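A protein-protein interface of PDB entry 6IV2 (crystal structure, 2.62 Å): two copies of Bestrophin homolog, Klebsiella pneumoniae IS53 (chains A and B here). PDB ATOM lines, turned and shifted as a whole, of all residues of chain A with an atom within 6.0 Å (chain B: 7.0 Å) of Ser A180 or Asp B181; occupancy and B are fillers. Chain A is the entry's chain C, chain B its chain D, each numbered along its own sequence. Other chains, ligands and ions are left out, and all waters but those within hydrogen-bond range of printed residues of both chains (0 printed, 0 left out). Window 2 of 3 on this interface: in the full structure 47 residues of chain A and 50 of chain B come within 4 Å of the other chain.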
ATOM      1  N   ARG A 174       2.885   2.429  29.376  1.00  0.00           N
ATOM      2  CA  ARG A 174       3.989   1.869  30.136  1.00  0.00           C
ATOM      3  C   ARG A 174       4.068   2.482  31.530  1.00  0.00           C
ATOM      4  O   ARG A 174       4.352   1.776  32.506  1.00  0.00           O
ATOM      5  CB  ARG A 174       5.297   2.070  29.382  1.00  0.00           C
ATOM      6  CG  ARG A 174       6.448   1.349  30.023  1.00  0.00           C
ATOM      7  CD  ARG A 174       7.772   1.831  29.496  1.00  0.00           C
ATOM      8  NE  ARG A 174       8.703   2.048  30.595  1.00  0.00           N
ATOM      9  CZ  ARG A 174       9.030   3.241  31.070  1.00  0.00           C
ATOM     10  NH1 ARG A 174       9.882   3.337  32.075  1.00  0.00           N
ATOM     11  NH2 ARG A 174       8.521   4.339  30.526  1.00  0.00           N
ATOM     12  N   GLY A 177       1.637   1.511  33.753  1.00  0.00           N
ATOM     13  CA  GLY A 177       2.052   0.221  34.256  1.00  0.00           C
ATOM     14  C   GLY A 177       1.392  -0.968  33.611  1.00  0.00           C
ATOM     15  O   GLY A 177       1.570  -2.090  34.097  1.00  0.00           O
ATOM     16  N   LYS A 178       0.629  -0.758  32.534  1.00  0.00           N
ATOM     17  CA  LYS A 178      -0.005  -1.862  31.818  1.00  0.00           C
ATOM     18  C   LYS A 178       0.907  -2.468  30.760  1.00  0.00           C
ATOM     19  O   LYS A 178       0.626  -3.559  30.262  1.00  0.00           O
ATOM     20  CB  LYS A 178      -1.330  -1.397  31.191  1.00  0.00           C
ATOM     21  CG  LYS A 178      -1.438   0.085  30.936  1.00  0.00           C
ATOM     22  CD  LYS A 178      -2.883   0.503  30.710  1.00  0.00           C
ATOM     23  CE  LYS A 178      -3.757   0.264  31.930  1.00  0.00           C
ATOM     24  NZ  LYS A 178      -5.114   0.880  31.751  1.00  0.00           N
ATOM     25  N   LEU A 179       1.982  -1.784  30.401  1.00  0.00           N
ATOM     26  CA  LEU A 179       3.051  -2.356  29.597  1.00  0.00           C
ATOM     27  C   LEU A 179       4.326  -2.391  30.424  1.00  0.00           C
ATOM     28  O   LEU A 179       4.708  -1.382  31.031  1.00  0.00           O
ATOM     29  CB  LEU A 179       3.308  -1.556  28.316  1.00  0.00           C
ATOM     30  CG  LEU A 179       2.269  -1.570  27.203  1.00  0.00           C
ATOM     31  CD1 LEU A 179       2.609  -0.486  26.187  1.00  0.00           C
ATOM     32  CD2 LEU A 179       2.211  -2.934  26.551  1.00  0.00           C
ATOM     33  N   SER A 180       4.970  -3.554  30.457  1.00  0.00           N
ATOM     34  CA  SER A 180       6.306  -3.689  31.003  1.00  0.00           C
ATOM     35  C   SER A 180       7.323  -3.156  29.998  1.00  0.00           C
ATOM     36  O   SER A 180       7.007  -2.912  28.832  1.00  0.00           O
ATOM     37  CB  SER A 180       6.591  -5.148  31.330  1.00  0.00           C
ATOM     38  OG  SER A 180       6.817  -5.872  30.134  1.00  0.00           O
ATOM     39  N   ASP A 181       8.566  -2.976  30.458  1.00  0.00           N
ATOM     40  CA  ASP A 181       9.627  -2.538  29.551  1.00  0.00           C
ATOM     41  C   ASP A 181       9.790  -3.491  28.369  1.00  0.00           C
ATOM     42  O   ASP A 181      10.060  -3.052  27.243  1.00  0.00           O
ATOM     43  CB  ASP A 181      10.944  -2.398  30.311  1.00  0.00           C
ATOM     44  CG  ASP A 181      10.954  -1.194  31.229  1.00  0.00           C
ATOM     45  OD1 ASP A 181      10.126  -0.288  31.008  1.00  0.00           O
ATOM     46  OD2 ASP A 181      11.779  -1.150  32.169  1.00  0.00           O
ATOM     47  N   ILE A 182       9.622  -4.795  28.596  1.00  0.00           N
ATOM     48  CA  ILE A 182       9.719  -5.772  27.514  1.00  0.00           C
ATOM     49  C   ILE A 182       8.618  -5.523  26.492  1.00  0.00           C
ATOM     50  O   ILE A 182       8.899  -5.165  25.343  1.00  0.00           O
ATOM     51  CB  ILE A 182       9.643  -7.224  28.026  1.00  0.00           C
ATOM     52  CG1 ILE A 182      10.721  -7.500  29.065  1.00  0.00           C
ATOM     53  CG2 ILE A 182       9.793  -8.193  26.874  1.00  0.00           C
ATOM     54  CD1 ILE A 182      12.071  -7.160  28.577  1.00  0.00           C
ATOM     55  N   THR A 183       7.358  -5.727  26.894  1.00  0.00           N
ATOM     56  CA  THR A 183       6.261  -5.574  25.942  1.00  0.00           C
ATOM     57  C   THR A 183       6.143  -4.147  25.435  1.00  0.00           C
ATOM     58  O   THR A 183       5.630  -3.943  24.335  1.00  0.00           O
ATOM     59  CB  THR A 183       4.922  -6.022  26.542  1.00  0.00           C
ATOM     60  OG1 THR A 183       4.540  -5.145  27.608  1.00  0.00           O
ATOM     61  CG2 THR A 183       5.014  -7.447  27.063  1.00  0.00           C
ATOM     62  N   TYR A 184       6.622  -3.154  26.184  1.00  0.00           N
ATOM     63  CA  TYR A 184       6.761  -1.832  25.586  1.00  0.00           C
ATOM     64  C   TYR A 184       7.727  -1.879  24.410  1.00  0.00           C
ATOM     65  O   TYR A 184       7.428  -1.365  23.327  1.00  0.00           O
ATOM     66  CB  TYR A 184       7.234  -0.800  26.610  1.00  0.00           C
ATOM     67  CG  TYR A 184       7.620   0.512  25.959  1.00  0.00           C
ATOM     68  CD1 TYR A 184       6.673   1.487  25.707  1.00  0.00           C
ATOM     69  CD2 TYR A 184       8.932   0.762  25.567  1.00  0.00           C
ATOM     70  CE1 TYR A 184       7.018   2.680  25.098  1.00  0.00           C
ATOM     71  CE2 TYR A 184       9.284   1.944  24.954  1.00  0.00           C
ATOM     72  CZ  TYR A 184       8.327   2.899  24.726  1.00  0.00           C
ATOM     73  OH  TYR A 184       8.691   4.074  24.116  1.00  0.00           O
ATOM     74  N   GLY A 185       8.898  -2.491  24.612  1.00  0.00           N
ATOM     75  CA  GLY A 185       9.916  -2.491  23.574  1.00  0.00           C
ATOM     76  C   GLY A 185       9.491  -3.233  22.319  1.00  0.00           C
ATOM     77  O   GLY A 185       9.836  -2.828  21.207  1.00  0.00           O
ATOM     78  N   LEU A 186       8.737  -4.329  22.475  1.00  0.00           N
ATOM     79  CA  LEU A 186       8.252  -5.054  21.301  1.00  0.00           C
ATOM     80  C   LEU A 186       7.439  -4.155  20.383  1.00  0.00           C
ATOM     81  O   LEU A 186       7.551  -4.251  19.158  1.00  0.00           O
ATOM     82  CB  LEU A 186       7.424  -6.277  21.709  1.00  0.00           C
ATOM     83  CG  LEU A 186       8.055  -7.259  22.685  1.00  0.00           C
ATOM     84  CD1 LEU A 186       7.016  -8.248  23.213  1.00  0.00           C
ATOM     85  CD2 LEU A 186       9.198  -7.969  22.001  1.00  0.00           C
ATOM     86  N   ARG B 174       0.852 -15.890  28.027  1.00  0.00           N
ATOM     87  CA  ARG B 174       1.558 -14.849  28.767  1.00  0.00           C
ATOM     88  C   ARG B 174       0.765 -14.406  29.989  1.00  0.00           C
ATOM     89  O   ARG B 174       1.328 -14.252  31.079  1.00  0.00           O
ATOM     90  CB  ARG B 174       1.849 -13.649  27.864  1.00  0.00           C
ATOM     91  CG  ARG B 174       2.892 -12.702  28.446  1.00  0.00           C
ATOM     92  CD  ARG B 174       2.845 -11.294  27.830  1.00  0.00           C
ATOM     93  NE  ARG B 174       2.069 -10.337  28.629  1.00  0.00           N
ATOM     94  CZ  ARG B 174       0.803 -10.009  28.375  1.00  0.00           C
ATOM     95  NH1 ARG B 174       0.184  -9.132  29.155  1.00  0.00           N
ATOM     96  NH2 ARG B 174       0.150 -10.550  27.337  1.00  0.00           N
ATOM     97  N   LEU B 179       4.181 -18.149  30.193  1.00  0.00           N
ATOM     98  CA  LEU B 179       5.261 -17.479  29.486  1.00  0.00           C
ATOM     99  C   LEU B 179       5.555 -16.160  30.181  1.00  0.00           C
ATOM    100  O   LEU B 179       4.640 -15.484  30.652  1.00  0.00           O
ATOM    101  CB  LEU B 179       4.910 -17.208  28.016  1.00  0.00           C
ATOM    102  CG  LEU B 179       4.745 -18.372  27.040  1.00  0.00           C
ATOM    103  CD1 LEU B 179       4.204 -17.869  25.708  1.00  0.00           C
ATOM    104  CD2 LEU B 179       6.064 -19.094  26.848  1.00  0.00           C
ATOM    105  N   SER B 180       6.830 -15.807  30.259  1.00  0.00           N
ATOM    106  CA  SER B 180       7.209 -14.483  30.713  1.00  0.00           C
ATOM    107  C   SER B 180       7.169 -13.523  29.529  1.00  0.00           C
ATOM    108  O   SER B 180       6.937 -13.919  28.383  1.00  0.00           O
ATOM    109  CB  SER B 180       8.593 -14.515  31.344  1.00  0.00           C
ATOM    110  OG  SER B 180       9.575 -14.784  30.360  1.00  0.00           O
ATOM    111  N   ASP B 181       7.398 -12.237  29.797  1.00  0.00           N
ATOM    112  CA  ASP B 181       7.481 -11.281  28.701  1.00  0.00           C
ATOM    113  C   ASP B 181       8.643 -11.609  27.772  1.00  0.00           C
ATOM    114  O   ASP B 181       8.548 -11.382  26.560  1.00  0.00           O
ATOM    115  CB  ASP B 181       7.613  -9.859  29.248  1.00  0.00           C
ATOM    116  CG  ASP B 181       6.320  -9.342  29.855  1.00  0.00           C
ATOM    117  OD1 ASP B 181       5.259  -9.963  29.630  1.00  0.00           O
ATOM    118  OD2 ASP B 181       6.365  -8.316  30.568  1.00  0.00           O
ATOM    119  N   ILE B 182       9.733 -12.162  28.311  1.00  0.00           N
ATOM    120  CA  ILE B 182      10.879 -12.509  27.472  1.00  0.00           C
ATOM    121  C   ILE B 182      10.506 -13.604  26.482  1.00  0.00           C
ATOM    122  O   ILE B 182      10.639 -13.437  25.265  1.00  0.00           O
ATOM    123  CB  ILE B 182      12.080 -12.926  28.338  1.00  0.00           C
ATOM    124  CG1 ILE B 182      12.614 -11.721  29.097  1.00  0.00           C
ATOM    125  CG2 ILE B 182      13.178 -13.495  27.465  1.00  0.00           C
ATOM    126  CD1 ILE B 182      12.739 -10.512  28.216  1.00  0.00           C
ATOM    127  N   THR B 183      10.032 -14.741  26.985  1.00  0.00           N
ATOM    128  CA  THR B 183       9.713 -15.843  26.093  1.00  0.00           C
ATOM    129  C   THR B 183       8.447 -15.588  25.294  1.00  0.00           C
ATOM    130  O   THR B 183       8.311 -16.134  24.196  1.00  0.00           O
ATOM    131  CB  THR B 183       9.602 -17.150  26.874  1.00  0.00           C
ATOM    132  OG1 THR B 183       8.532 -17.059  27.817  1.00  0.00           O
ATOM    133  CG2 THR B 183      10.914 -17.417  27.617  1.00  0.00           C
ATOM    134  N   TYR B 184       7.532 -14.754  25.788  1.00  0.00           N
ATOM    135  CA  TYR B 184       6.480 -14.259  24.909  1.00  0.00           C
ATOM    136  C   TYR B 184       7.086 -13.565  23.697  1.00  0.00           C
ATOM    137  O   TYR B 184       6.692 -13.826  22.554  1.00  0.00           O
ATOM    138  CB  TYR B 184       5.551 -13.299  25.652  1.00  0.00           C
ATOM    139  CG  TYR B 184       4.557 -12.649  24.716  1.00  0.00           C
ATOM    140  CD1 TYR B 184       3.430 -13.340  24.284  1.00  0.00           C
ATOM    141  CD2 TYR B 184       4.755 -11.359  24.238  1.00  0.00           C
ATOM    142  CE1 TYR B 184       2.525 -12.766  23.414  1.00  0.00           C
ATOM    143  CE2 TYR B 184       3.847 -10.774  23.368  1.00  0.00           C
ATOM    144  CZ  TYR B 184       2.738 -11.482  22.962  1.00  0.00           C
ATOM    145  OH  TYR B 184       1.839 -10.905  22.096  1.00  0.00           O
ATOM    146  N   GLY B 185       8.067 -12.688  23.933  1.00  0.00           N
ATOM    147  CA  GLY B 185       8.669 -11.938  22.842  1.00  0.00           C
ATOM    148  C   GLY B 185       9.435 -12.813  21.868  1.00  0.00           C
ATOM    149  O   GLY B 185       9.420 -12.568  20.659  1.00  0.00           O
ATOM    150  N   LEU B 186      10.119 -13.842  22.376  1.00  0.00           N
ATOM    151  CA  LEU B 186      10.803 -14.769  21.479  1.00  0.00           C
ATOM    152  C   LEU B 186       9.826 -15.396  20.495  1.00  0.00           C
ATOM    153  O   LEU B 186      10.146 -15.575  19.317  1.00  0.00           O
ATOM    154  CB  LEU B 186      11.523 -15.850  22.281  1.00  0.00           C
ATOM    155  CG  LEU B 186      12.640 -15.372  23.202  1.00  0.00           C
ATOM    156  CD1 LEU B 186      13.131 -16.510  24.089  1.00  0.00           C
ATOM    157  CD2 LEU B 186      13.768 -14.796  22.377  1.00  0.00           C
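Of the printed residues of chain B, Ser A180 touches Asp B181 (2.5 Å).
Of the printed residues of chain B, Ile A182 touches Asp B181 and Ile B182.
Printed residues of chain B within 4 Å of Thr A183: Asp B181 (3.6 Å).
Printed residues of chain B within 4 Å of Leu A186: Tyr B184 (3.98 Å).
Arg B174 touches none of the printed residues of chain A.
Leu B179 touches none of the printed residues of chain A.
Of the printed residues of chain A, Ile B182 touches Ile A182.
Of the printed residues of chain A, Tyr B184 touches Leu A186.
The nearest residue of chain B that does not touch Ser A180 is Arg B174 (6.7 Å).
N of Ile A182 lies close to OG of Ser A180.
The side-chain hydroxyl of Ser A180 lies within hydrogen-bond range of the backbone NH of Thr A183.
The side-chain carboxylate (OD1) of Asp B181 is in salt-bridge range of the guanidinium group (NE) of Arg B174.
The backbone NH of Ile B182 sits close to the side-chain hydroxyl of Ser B180 (3.3 Å).
Ser A180 touches Asp B181, but with the chains exchanged Asp A181 does not touch Ser B180 (10.4 Å).
Ile A182 touches Asp B181, but with the chains exchanged Asp A181 does not touch Ile B182 (7.6 Å).
Ile A182 touches its own counterpart, Ile B182.
Leu A186 touches Tyr B184, but with the chains exchanged Tyr A184 does not touch Leu B186 (11.9 Å).
Of the 5 pairs that touch across the chains among the printed residues, 1 has its exchanged pair printed and touching as well.
Printed residues of chain A that touch a printed residue of chain B: Ser A180, Ile A182, Thr A183 and Leu A186.
Hydrophobic or aromatic side chains of chain A that line the printed part of chain B: Ile A182 and Leu A186.
Hydrophobic or aromatic side chains of chain B within 4 Å of the printed part of chain A: Ile B182 and Tyr B184.
Among the printed residues, 5 pairs touch across the chains.
Among the printed residues, no Asp or Glu carboxylate lies within 4 Å of a Lys or Arg side-chain nitrogen of the other chain.
Among the printed residues, merely in contact across the chains: Ile A182 with Asp B181 (3.4 Å), Ile A182 with Ile B182 (3.4 Å), Thr A183 with Asp B181 (3.6 Å) and Leu A186 with Tyr B184 (3.98 Å).
The side-chain hydroxyl (OG) of Ser A180 is in hydrogen-bond range of the side-chain carboxylate (OD2) of Asp B181 (2.5 Å).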
